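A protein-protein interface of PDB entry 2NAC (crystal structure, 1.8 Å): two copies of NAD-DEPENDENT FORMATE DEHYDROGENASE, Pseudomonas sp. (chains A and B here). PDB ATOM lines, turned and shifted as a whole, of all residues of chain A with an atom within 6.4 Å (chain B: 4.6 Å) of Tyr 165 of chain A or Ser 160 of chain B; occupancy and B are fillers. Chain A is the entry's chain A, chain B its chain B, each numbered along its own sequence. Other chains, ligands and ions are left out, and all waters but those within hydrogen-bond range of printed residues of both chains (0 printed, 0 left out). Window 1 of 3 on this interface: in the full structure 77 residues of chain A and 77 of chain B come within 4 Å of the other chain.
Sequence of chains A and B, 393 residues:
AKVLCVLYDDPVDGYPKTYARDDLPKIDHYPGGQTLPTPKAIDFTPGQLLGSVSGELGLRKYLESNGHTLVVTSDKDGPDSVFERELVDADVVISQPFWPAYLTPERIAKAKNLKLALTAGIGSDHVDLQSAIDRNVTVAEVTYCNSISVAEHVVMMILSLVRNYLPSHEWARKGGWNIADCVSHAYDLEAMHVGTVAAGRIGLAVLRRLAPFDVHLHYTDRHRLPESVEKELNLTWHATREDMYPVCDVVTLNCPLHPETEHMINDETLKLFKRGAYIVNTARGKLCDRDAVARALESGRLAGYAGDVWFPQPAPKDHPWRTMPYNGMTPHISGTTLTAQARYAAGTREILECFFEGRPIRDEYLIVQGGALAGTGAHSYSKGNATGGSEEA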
ATOM      1  N   MET A 156      32.341  -2.674 -12.025  1.00  0.00           N
ATOM      2  CA  MET A 156      32.065  -1.210 -11.928  1.00  0.00           C
ATOM      3  C   MET A 156      31.304  -0.732 -13.137  1.00  0.00           C
ATOM      4  O   MET A 156      30.324  -0.004 -13.047  1.00  0.00           O
ATOM      5  CB  MET A 156      33.398  -0.501 -11.807  1.00  0.00           C
ATOM      6  CG  MET A 156      33.332   1.025 -11.839  1.00  0.00           C
ATOM      7  SD  MET A 156      34.959   1.726 -11.869  1.00  0.00           S
ATOM      8  CE  MET A 156      35.344   1.548 -13.581  1.00  0.00           C
ATOM      9  N   LEU A 159      27.544  -2.147 -13.336  1.00  0.00           N
ATOM     10  CA  LEU A 159      26.706  -1.363 -12.373  1.00  0.00           C
ATOM     11  C   LEU A 159      26.429   0.016 -12.921  1.00  0.00           C
ATOM     12  O   LEU A 159      25.253   0.455 -12.843  1.00  0.00           O
ATOM     13  CB  LEU A 159      27.404  -1.334 -11.019  1.00  0.00           C
ATOM     14  CG  LEU A 159      27.213  -2.613 -10.215  1.00  0.00           C
ATOM     15  CD1 LEU A 159      28.240  -2.538  -9.068  1.00  0.00           C
ATOM     16  CD2 LEU A 159      25.826  -2.836  -9.658  1.00  0.00           C
ATOM     17  N   SER A 160      27.420   0.697 -13.393  1.00  0.00           N
ATOM     18  CA  SER A 160      27.330   2.020 -13.904  1.00  0.00           C
ATOM     19  C   SER A 160      26.366   2.099 -15.067  1.00  0.00           C
ATOM     20  O   SER A 160      25.546   3.041 -15.156  1.00  0.00           O
ATOM     21  CB  SER A 160      28.652   2.682 -14.274  1.00  0.00           C
ATOM     22  OG  SER A 160      29.411   2.650 -13.035  1.00  0.00           O
ATOM     23  N   LEU A 161      26.465   1.154 -16.036  1.00  0.00           N
ATOM     24  CA  LEU A 161      25.553   1.167 -17.171  1.00  0.00           C
ATOM     25  C   LEU A 161      24.111   0.875 -16.781  1.00  0.00           C
ATOM     26  O   LEU A 161      23.167   1.562 -17.260  1.00  0.00           O
ATOM     27  CB  LEU A 161      25.961   0.114 -18.240  1.00  0.00           C
ATOM     28  CG  LEU A 161      27.218   0.462 -19.028  1.00  0.00           C
ATOM     29  CD1 LEU A 161      27.406  -0.756 -19.970  1.00  0.00           C
ATOM     30  CD2 LEU A 161      27.106   1.750 -19.817  1.00  0.00           C
ATOM     31  N   VAL A 162      23.921  -0.149 -15.970  1.00  0.00           N
ATOM     32  CA  VAL A 162      22.578  -0.568 -15.582  1.00  0.00           C
ATOM     33  C   VAL A 162      21.810   0.539 -14.772  1.00  0.00           C
ATOM     34  O   VAL A 162      20.633   0.810 -15.029  1.00  0.00           O
ATOM     35  CB  VAL A 162      22.661  -1.871 -14.825  1.00  0.00           C
ATOM     36  CG1 VAL A 162      21.388  -2.352 -14.210  1.00  0.00           C
ATOM     37  CG2 VAL A 162      23.137  -3.026 -15.746  1.00  0.00           C
ATOM     38  N   ARG A 163      22.517   1.180 -13.879  1.00  0.00           N
ATOM     39  CA  ARG A 163      21.956   2.182 -12.965  1.00  0.00           C
ATOM     40  C   ARG A 163      22.000   3.554 -13.548  1.00  0.00           C
ATOM     41  O   ARG A 163      21.617   4.517 -12.890  1.00  0.00           O
ATOM     42  CB  ARG A 163      22.630   2.063 -11.602  1.00  0.00           C
ATOM     43  CG  ARG A 163      22.543   0.712 -10.910  1.00  0.00           C
ATOM     44  CD  ARG A 163      23.050   0.634  -9.470  1.00  0.00           C
ATOM     45  NE  ARG A 163      22.281   1.594  -8.674  1.00  0.00           N
ATOM     46  CZ  ARG A 163      21.026   1.323  -8.294  1.00  0.00           C
ATOM     47  NH1 ARG A 163      20.440   0.166  -8.504  1.00  0.00           N
ATOM     48  NH2 ARG A 163      20.331   2.355  -7.745  1.00  0.00           N
ATOM     49  N   ASN A 164      22.493   3.735 -14.765  1.00  0.00           N
ATOM     50  CA  ASN A 164      22.612   4.991 -15.455  1.00  0.00           C
ATOM     51  C   ASN A 164      23.370   6.021 -14.705  1.00  0.00           C
ATOM     52  O   ASN A 164      23.086   7.222 -14.656  1.00  0.00           O
ATOM     53  CB  ASN A 164      21.208   5.506 -15.824  1.00  0.00           C
ATOM     54  CG  ASN A 164      21.200   6.418 -16.999  1.00  0.00           C
ATOM     55  OD1 ASN A 164      21.857   6.235 -18.009  1.00  0.00           O
ATOM     56  ND2 ASN A 164      20.317   7.469 -16.922  1.00  0.00           N
ATOM     57  N   TYR A 165      24.524   5.688 -14.105  1.00  0.00           N
ATOM     58  CA  TYR A 165      25.337   6.545 -13.312  1.00  0.00           C
ATOM     59  C   TYR A 165      25.935   7.712 -13.988  1.00  0.00           C
ATOM     60  O   TYR A 165      26.006   8.865 -13.486  1.00  0.00           O
ATOM     61  CB  TYR A 165      26.539   5.761 -12.676  1.00  0.00           C
ATOM     62  CG  TYR A 165      27.342   6.415 -11.621  1.00  0.00           C
ATOM     63  CD1 TYR A 165      26.948   7.505 -10.820  1.00  0.00           C
ATOM     64  CD2 TYR A 165      28.623   5.892 -11.323  1.00  0.00           C
ATOM     65  CE1 TYR A 165      27.753   8.014  -9.864  1.00  0.00           C
ATOM     66  CE2 TYR A 165      29.411   6.398 -10.328  1.00  0.00           C
ATOM     67  CZ  TYR A 165      28.995   7.473  -9.570  1.00  0.00           C
ATOM     68  OH  TYR A 165      29.789   7.975  -8.592  1.00  0.00           O
ATOM     69  N   LEU A 166      26.503   7.531 -15.222  1.00  0.00           N
ATOM     70  CA  LEU A 166      27.188   8.625 -15.890  1.00  0.00           C
ATOM     71  C   LEU A 166      26.301   9.849 -16.210  1.00  0.00           C
ATOM     72  O   LEU A 166      26.670  10.970 -15.837  1.00  0.00           O
ATOM     73  CB  LEU A 166      28.100   8.103 -17.023  1.00  0.00           C
ATOM     74  CG  LEU A 166      29.163   7.057 -16.589  1.00  0.00           C
ATOM     75  CD1 LEU A 166      29.915   6.578 -17.874  1.00  0.00           C
ATOM     76  CD2 LEU A 166      30.178   7.590 -15.615  1.00  0.00           C
ATOM     77  N   PRO A 167      25.203   9.646 -16.843  1.00  0.00           N
ATOM     78  CA  PRO A 167      24.247  10.746 -17.109  1.00  0.00           C
ATOM     79  C   PRO A 167      23.729  11.303 -15.751  1.00  0.00           C
ATOM     80  O   PRO A 167      23.627  12.514 -15.660  1.00  0.00           O
ATOM     81  CB  PRO A 167      23.090  10.145 -17.938  1.00  0.00           C
ATOM     82  CG  PRO A 167      23.794   8.941 -18.552  1.00  0.00           C
ATOM     83  CD  PRO A 167      24.686   8.418 -17.417  1.00  0.00           C
ATOM     84  N   SER A 168      23.463  10.538 -14.736  1.00  0.00           N
ATOM     85  CA  SER A 168      23.025  11.037 -13.444  1.00  0.00           C
ATOM     86  C   SER A 168      24.066  11.893 -12.861  1.00  0.00           C
ATOM     87  O   SER A 168      23.822  12.964 -12.291  1.00  0.00           O
ATOM     88  CB  SER A 168      22.695   9.883 -12.521  1.00  0.00           C
ATOM     89  OG  SER A 168      21.680   9.133 -13.103  1.00  0.00           O
ATOM     90  N   HIS A 169      25.369  11.529 -12.912  1.00  0.00           N
ATOM     91  CA  HIS A 169      26.423  12.339 -12.388  1.00  0.00           C
ATOM     92  C   HIS A 169      26.489  13.650 -13.157  1.00  0.00           C
ATOM     93  O   HIS A 169      26.809  14.724 -12.584  1.00  0.00           O
ATOM     94  CB  HIS A 169      27.785  11.608 -12.374  1.00  0.00           C
ATOM     95  CG  HIS A 169      28.901  12.480 -11.915  1.00  0.00           C
ATOM     96  ND1 HIS A 169      29.053  12.904 -10.612  1.00  0.00           N
ATOM     97  CD2 HIS A 169      29.918  12.988 -12.619  1.00  0.00           C
ATOM     98  CE1 HIS A 169      30.147  13.640 -10.578  1.00  0.00           C
ATOM     99  NE2 HIS A 169      30.695  13.709 -11.759  1.00  0.00           N
ATOM    100  N   GLU A 170      26.326  13.698 -14.466  1.00  0.00           N
ATOM    101  CA  GLU A 170      26.392  14.923 -15.239  1.00  0.00           C
ATOM    102  C   GLU A 170      25.282  15.934 -14.797  1.00  0.00           C
ATOM    103  O   GLU A 170      25.635  17.123 -14.798  1.00  0.00           O
ATOM    104  CB  GLU A 170      26.357  14.726 -16.775  1.00  0.00           C
ATOM    105  CG  GLU A 170      27.644  13.990 -17.177  1.00  0.00           C
ATOM    106  CD  GLU A 170      28.904  14.833 -16.928  1.00  0.00           C
ATOM    107  OE1 GLU A 170      28.707  15.965 -17.473  1.00  0.00           O
ATOM    108  OE2 GLU A 170      29.922  14.433 -16.302  1.00  0.00           O
ATOM    109  N   MET B 156      28.707   0.517  -6.453  1.00  0.00           N
ATOM    110  CA  MET B 156      29.040   1.192  -7.679  1.00  0.00           C
ATOM    111  C   MET B 156      29.926   2.359  -7.451  1.00  0.00           C
ATOM    112  O   MET B 156      30.896   2.665  -8.116  1.00  0.00           O
ATOM    113  CB  MET B 156      27.780   1.589  -8.456  1.00  0.00           C
ATOM    114  CG  MET B 156      27.956   2.407  -9.676  1.00  0.00           C
ATOM    115  SD  MET B 156      26.298   2.899 -10.303  1.00  0.00           S
ATOM    116  CE  MET B 156      25.936   4.242  -9.195  1.00  0.00           C
ATOM    117  N   MET B 157      29.463   3.210  -6.439  1.00  0.00           N
ATOM    118  CA  MET B 157      30.222   4.380  -6.079  1.00  0.00           C
ATOM    119  C   MET B 157      31.592   4.114  -5.401  1.00  0.00           C
ATOM    120  O   MET B 157      32.502   4.830  -5.719  1.00  0.00           O
ATOM    121  CB  MET B 157      29.335   5.298  -5.138  1.00  0.00           C
ATOM    122  CG  MET B 157      28.262   6.019  -5.998  1.00  0.00           C
ATOM    123  SD  MET B 157      27.126   6.952  -4.797  1.00  0.00           S
ATOM    124  CE  MET B 157      26.460   8.054  -6.050  1.00  0.00           C
ATOM    125  N   ILE B 158      31.634   3.098  -4.596  1.00  0.00           N
ATOM    126  CA  ILE B 158      32.930   2.739  -3.973  1.00  0.00           C
ATOM    127  C   ILE B 158      33.918   2.376  -5.101  1.00  0.00           C
ATOM    128  O   ILE B 158      34.994   2.973  -5.111  1.00  0.00           O
ATOM    129  CB  ILE B 158      32.713   1.559  -3.057  1.00  0.00           C
ATOM    130  CG1 ILE B 158      31.978   1.999  -1.762  1.00  0.00           C
ATOM    131  CG2 ILE B 158      34.122   0.961  -2.680  1.00  0.00           C
ATOM    132  CD1 ILE B 158      31.620   0.849  -0.862  1.00  0.00           C
ATOM    133  N   LEU B 159      33.510   1.466  -5.969  1.00  0.00           N
ATOM    134  CA  LEU B 159      34.389   1.104  -7.111  1.00  0.00           C
ATOM    135  C   LEU B 159      34.782   2.262  -7.932  1.00  0.00           C
ATOM    136  O   LEU B 159      35.912   2.544  -8.275  1.00  0.00           O
ATOM    137  CB  LEU B 159      33.690   0.070  -7.988  1.00  0.00           C
ATOM    138  CG  LEU B 159      33.588  -1.340  -7.417  1.00  0.00           C
ATOM    139  CD1 LEU B 159      32.647  -2.276  -8.136  1.00  0.00           C
ATOM    140  CD2 LEU B 159      35.010  -1.981  -7.454  1.00  0.00           C
ATOM    141  N   SER B 160      33.776   3.144  -8.289  1.00  0.00           N
ATOM    142  CA  SER B 160      34.086   4.290  -9.101  1.00  0.00           C
ATOM    143  C   SER B 160      35.014   5.269  -8.503  1.00  0.00           C
ATOM    144  O   SER B 160      35.855   5.831  -9.214  1.00  0.00           O
ATOM    145  CB  SER B 160      32.744   4.979  -9.530  1.00  0.00           C
ATOM    146  OG  SER B 160      31.944   4.041 -10.181  1.00  0.00           O
ATOM    147  N   LEU B 161      34.913   5.542  -7.206  1.00  0.00           N
ATOM    148  CA  LEU B 161      35.841   6.417  -6.539  1.00  0.00           C
ATOM    149  C   LEU B 161      37.317   5.874  -6.471  1.00  0.00           C
ATOM    150  O   LEU B 161      38.216   6.632  -6.805  1.00  0.00           O
ATOM    151  CB  LEU B 161      35.438   6.721  -5.096  1.00  0.00           C
ATOM    152  CG  LEU B 161      34.150   7.598  -4.856  1.00  0.00           C
ATOM    153  CD1 LEU B 161      33.901   7.706  -3.390  1.00  0.00           C
ATOM    154  CD2 LEU B 161      34.248   8.883  -5.605  1.00  0.00           C
ATOM    155  N   VAL B 162      37.387   4.639  -6.029  1.00  0.00           N
ATOM    156  CA  VAL B 162      38.730   3.987  -5.831  1.00  0.00           C
ATOM    157  C   VAL B 162      39.460   3.874  -7.157  1.00  0.00           C
ATOM    158  O   VAL B 162      40.639   4.221  -7.283  1.00  0.00           O
ATOM    159  CB  VAL B 162      38.508   2.692  -5.066  1.00  0.00           C
ATOM    160  CG1 VAL B 162      39.798   1.872  -5.073  1.00  0.00           C
ATOM    161  CG2 VAL B 162      37.985   2.862  -3.651  1.00  0.00           C
ATOM    162  N   ARG B 163      38.767   3.484  -8.206  1.00  0.00           N
ATOM    163  CA  ARG B 163      39.280   3.307  -9.553  1.00  0.00           C
ATOM    164  C   ARG B 163      39.359   4.514 -10.444  1.00  0.00           C
ATOM    165  O   ARG B 163      39.854   4.495 -11.587  1.00  0.00           O
ATOM    166  CB  ARG B 163      38.615   2.088 -10.155  1.00  0.00           C
ATOM    167  CG  ARG B 163      38.579   0.728  -9.455  1.00  0.00           C
ATOM    168  CD  ARG B 163      38.061  -0.490 -10.185  1.00  0.00           C
ATOM    169  NE  ARG B 163      38.822  -0.604 -11.454  1.00  0.00           N
ATOM    170  CZ  ARG B 163      40.059  -1.177 -11.512  1.00  0.00           C
ATOM    171  NH1 ARG B 163      40.545  -1.702 -10.424  1.00  0.00           N
ATOM    172  NH2 ARG B 163      40.705  -1.030 -12.608  1.00  0.00           N
ATOM    173  N   ASN B 164      38.913   5.720  -9.973  1.00  0.00           N
ATOM    174  CA  ASN B 164      38.938   6.982 -10.655  1.00  0.00           C
ATOM    175  C   ASN B 164      38.192   7.005 -11.986  1.00  0.00           C
ATOM    176  O   ASN B 164      38.617   7.554 -13.008  1.00  0.00           O
ATOM    177  CB  ASN B 164      40.386   7.460 -10.848  1.00  0.00           C
ATOM    178  CG  ASN B 164      40.557   8.936 -10.919  1.00  0.00           C
ATOM    179  OD1 ASN B 164      39.836   9.651 -10.208  1.00  0.00           O
ATOM    180  ND2 ASN B 164      41.452   9.402 -11.748  1.00  0.00           N
ATOM    181  N   TYR B 165      36.993   6.375 -11.939  1.00  0.00           N
ATOM    182  CA  TYR B 165      36.188   6.223 -13.129  1.00  0.00           C
ATOM    183  C   TYR B 165      35.704   7.466 -13.799  1.00  0.00           C
ATOM    184  O   TYR B 165      35.793   7.640 -14.986  1.00  0.00           O
ATOM    185  CB  TYR B 165      35.012   5.318 -12.847  1.00  0.00           C
ATOM    186  CG  TYR B 165      34.194   4.837 -14.023  1.00  0.00           C
ATOM    187  CD1 TYR B 165      34.650   4.793 -15.317  1.00  0.00           C
ATOM    188  CD2 TYR B 165      32.897   4.414 -13.765  1.00  0.00           C
ATOM    189  CE1 TYR B 165      33.829   4.306 -16.330  1.00  0.00           C
ATOM    190  CE2 TYR B 165      32.108   3.872 -14.763  1.00  0.00           C
ATOM    191  CZ  TYR B 165      32.606   3.831 -16.066  1.00  0.00           C
ATOM    192  OH  TYR B 165      31.746   3.328 -16.989  1.00  0.00           O
ATOM    193  N   LEU B 166      35.154   8.348 -12.961  1.00  0.00           N
ATOM    194  CA  LEU B 166      34.561   9.592 -13.530  1.00  0.00           C
ATOM    195  C   LEU B 166      35.499  10.450 -14.283  1.00  0.00           C
ATOM    196  O   LEU B 166      35.201  10.730 -15.457  1.00  0.00           O
ATOM    197  CB  LEU B 166      33.660  10.230 -12.472  1.00  0.00           C
ATOM    198  CG  LEU B 166      32.527   9.387 -11.930  1.00  0.00           C
ATOM    199  CD1 LEU B 166      31.751  10.175 -10.856  1.00  0.00           C
ATOM    200  CD2 LEU B 166      31.550   8.953 -12.975  1.00  0.00           C
ATOM    201  N   ALA B 306      31.340  10.328  -2.445  1.00  0.00           N
ATOM    202  CA  ALA B 306      30.231  10.131  -3.319  1.00  0.00           C
ATOM    203  C   ALA B 306      28.961   9.806  -2.466  1.00  0.00           C
ATOM    204  O   ALA B 306      28.981   9.227  -1.412  1.00  0.00           O
ATOM    205  CB  ALA B 306      30.367   9.072  -4.362  1.00  0.00           C
ATOM    206  N   GLY B 328      31.745  11.855  -6.653  1.00  0.00           N
ATOM    207  CA  GLY B 328      30.982  10.996  -7.526  1.00  0.00           C
ATOM    208  C   GLY B 328      29.477  11.148  -7.312  1.00  0.00           C
ATOM    209  O   GLY B 328      28.705  10.210  -7.293  1.00  0.00           O
ATOM    210  N   THR B 330      25.479  12.061  -7.367  1.00  0.00           N
ATOM    211  CA  THR B 330      24.285  12.035  -8.250  1.00  0.00           C
ATOM    212  C   THR B 330      23.151  12.795  -7.448  1.00  0.00           C
ATOM    213  O   THR B 330      23.246  12.927  -6.228  1.00  0.00           O
ATOM    214  CB  THR B 330      23.676  10.677  -8.533  1.00  0.00           C
ATOM    215  OG1 THR B 330      23.168   9.973  -7.384  1.00  0.00           O
ATOM    216  CG2 THR B 330      24.691   9.778  -9.315  1.00  0.00           C
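The side-chain hydroxyl (OH) of Tyr 165 of chain A is in hydrogen-bond range of the backbone carbonyl oxygen (O) of Gly 328 of chain B, 2.8 Å away. O of Leu 159 of chain A lies close to SD of Met 156 of chain B (3.7 Å).
The backbone carbonyl oxygen (O) of Met 156 of chain A lies within hydrogen-bond range of the side-chain hydroxyl (OG) of Ser 160 of chain A. The backbone carbonyl oxygen (O) of Ser 160 of chain A sits at hydrogen-bond distance from the backbone NH (N) of Tyr 165 of chain A, at 3.0 Å. OG of Ser 168 of chain A sits at hydrogen-bond distance from O of Asn 164 of chain A (2.8 Å). OG of Ser 160 of chain B sits at hydrogen-bond distance from O of Met 156 of chain B. N of Tyr 165 of chain B sits at hydrogen-bond distance from O of Ser 160 of chain B, 3.0 Å away.
Among the printed residues, pairs that only touch across the chains: Met 156 of chain A with Leu 159 of chain B, Met 156 of chain A with Ser 160 of chain B, Met 156 of chain A with Tyr 165 of chain B, Ser 160 of chain A with Met 156 of chain B, Ser 160 of chain A with Tyr 165 of chain B, Arg 163 of chain A with Met 156 of chain B, Tyr 165 of chain A with Met 156 of chain B, Tyr 165 of chain A with Met 157 of chain B, Tyr 165 of chain A with Ser 160 of chain B, Tyr 165 of chain A with Leu 166 of chain B, Tyr 165 of chain A with Thr 330 of chain B, Leu 166 of chain A with Tyr 165 of chain B, Leu 166 of chain A with Leu 166 of chain B, Ser 168 of chain A with Thr 330 of chain B, His 169 of chain A with Leu 166 of chain B and His 169 of chain A with Gly 328 of chain B.
Tyr 165 of chain A touches just these residues of chain B: Met 156, Met 157, Ser 160, Leu 166, Gly 328 and Thr 330. Printed residues of chain A within 4 Å of Gly 328 of chain B: Tyr 165 (2.8 Å) and His 169 (3.8 Å). Printed residues of chain A within 4 Å of Thr 330 of chain B: Tyr 165 (3.5 Å) and Ser 168 (3.8 Å). Printed residues of chain A within 4 Å of Leu 159 of chain B: Met 156 (3.8 Å). Asn 164 of chain B touches none of the printed residues of chain A. Pro 167 of chain A touches none of the printed residues of chain B. The nearest residue of chain A that does not touch Ser 160 of chain B is Ser 160 of chain A (4.1 Å). The nearest printed residue of chain A that does not touch Leu 166 of chain B is Glu 170 of chain A (6.5 Å).
Printed residues of chain B that touch a printed residue of chain A: Met 156, Met 157, Leu 159, Ser 160, Tyr 165, Leu 166, Gly 328 and Thr 330. Hydrophobic or aromatic side chains of chain B within 4 Å of the printed part of chain A: Met 156, Met 157, Leu 159, Tyr 165 and Leu 166. Hydrophobic or aromatic side chains of chain A within 4 Å of the printed part of chain B: Met 156, Leu 159, Tyr 165, Leu 166 and His 169. Among the printed residues, 18 pairs touch across the chains. Among the printed residues, no Asp or Glu carboxylate lies within 4 Å of a Lys or Arg side-chain nitrogen of the other chain.
Met 156 of chain A touches Tyr 165 of chain B, and with the chains exchanged Tyr 165 of chain A touches Met 156 of chain B. Ser 160 of chain A touches Tyr 165 of chain B, and with the chains exchanged Tyr 165 of chain A touches Ser 160 of chain B. Arg 163 of chain A touches Met 156 of chain B, but with the chains exchanged Met 156 of chain A does not touch Arg 163 of chain B (4.1 Å). Tyr 165 of chain A touches Leu 166 of chain B, and with the chains exchanged Leu 166 of chain A touches Tyr 165 of chain B. Of the 18 pairs that touch across the chains among the printed residues, 11 have their exchanged pair printed and touching as well.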
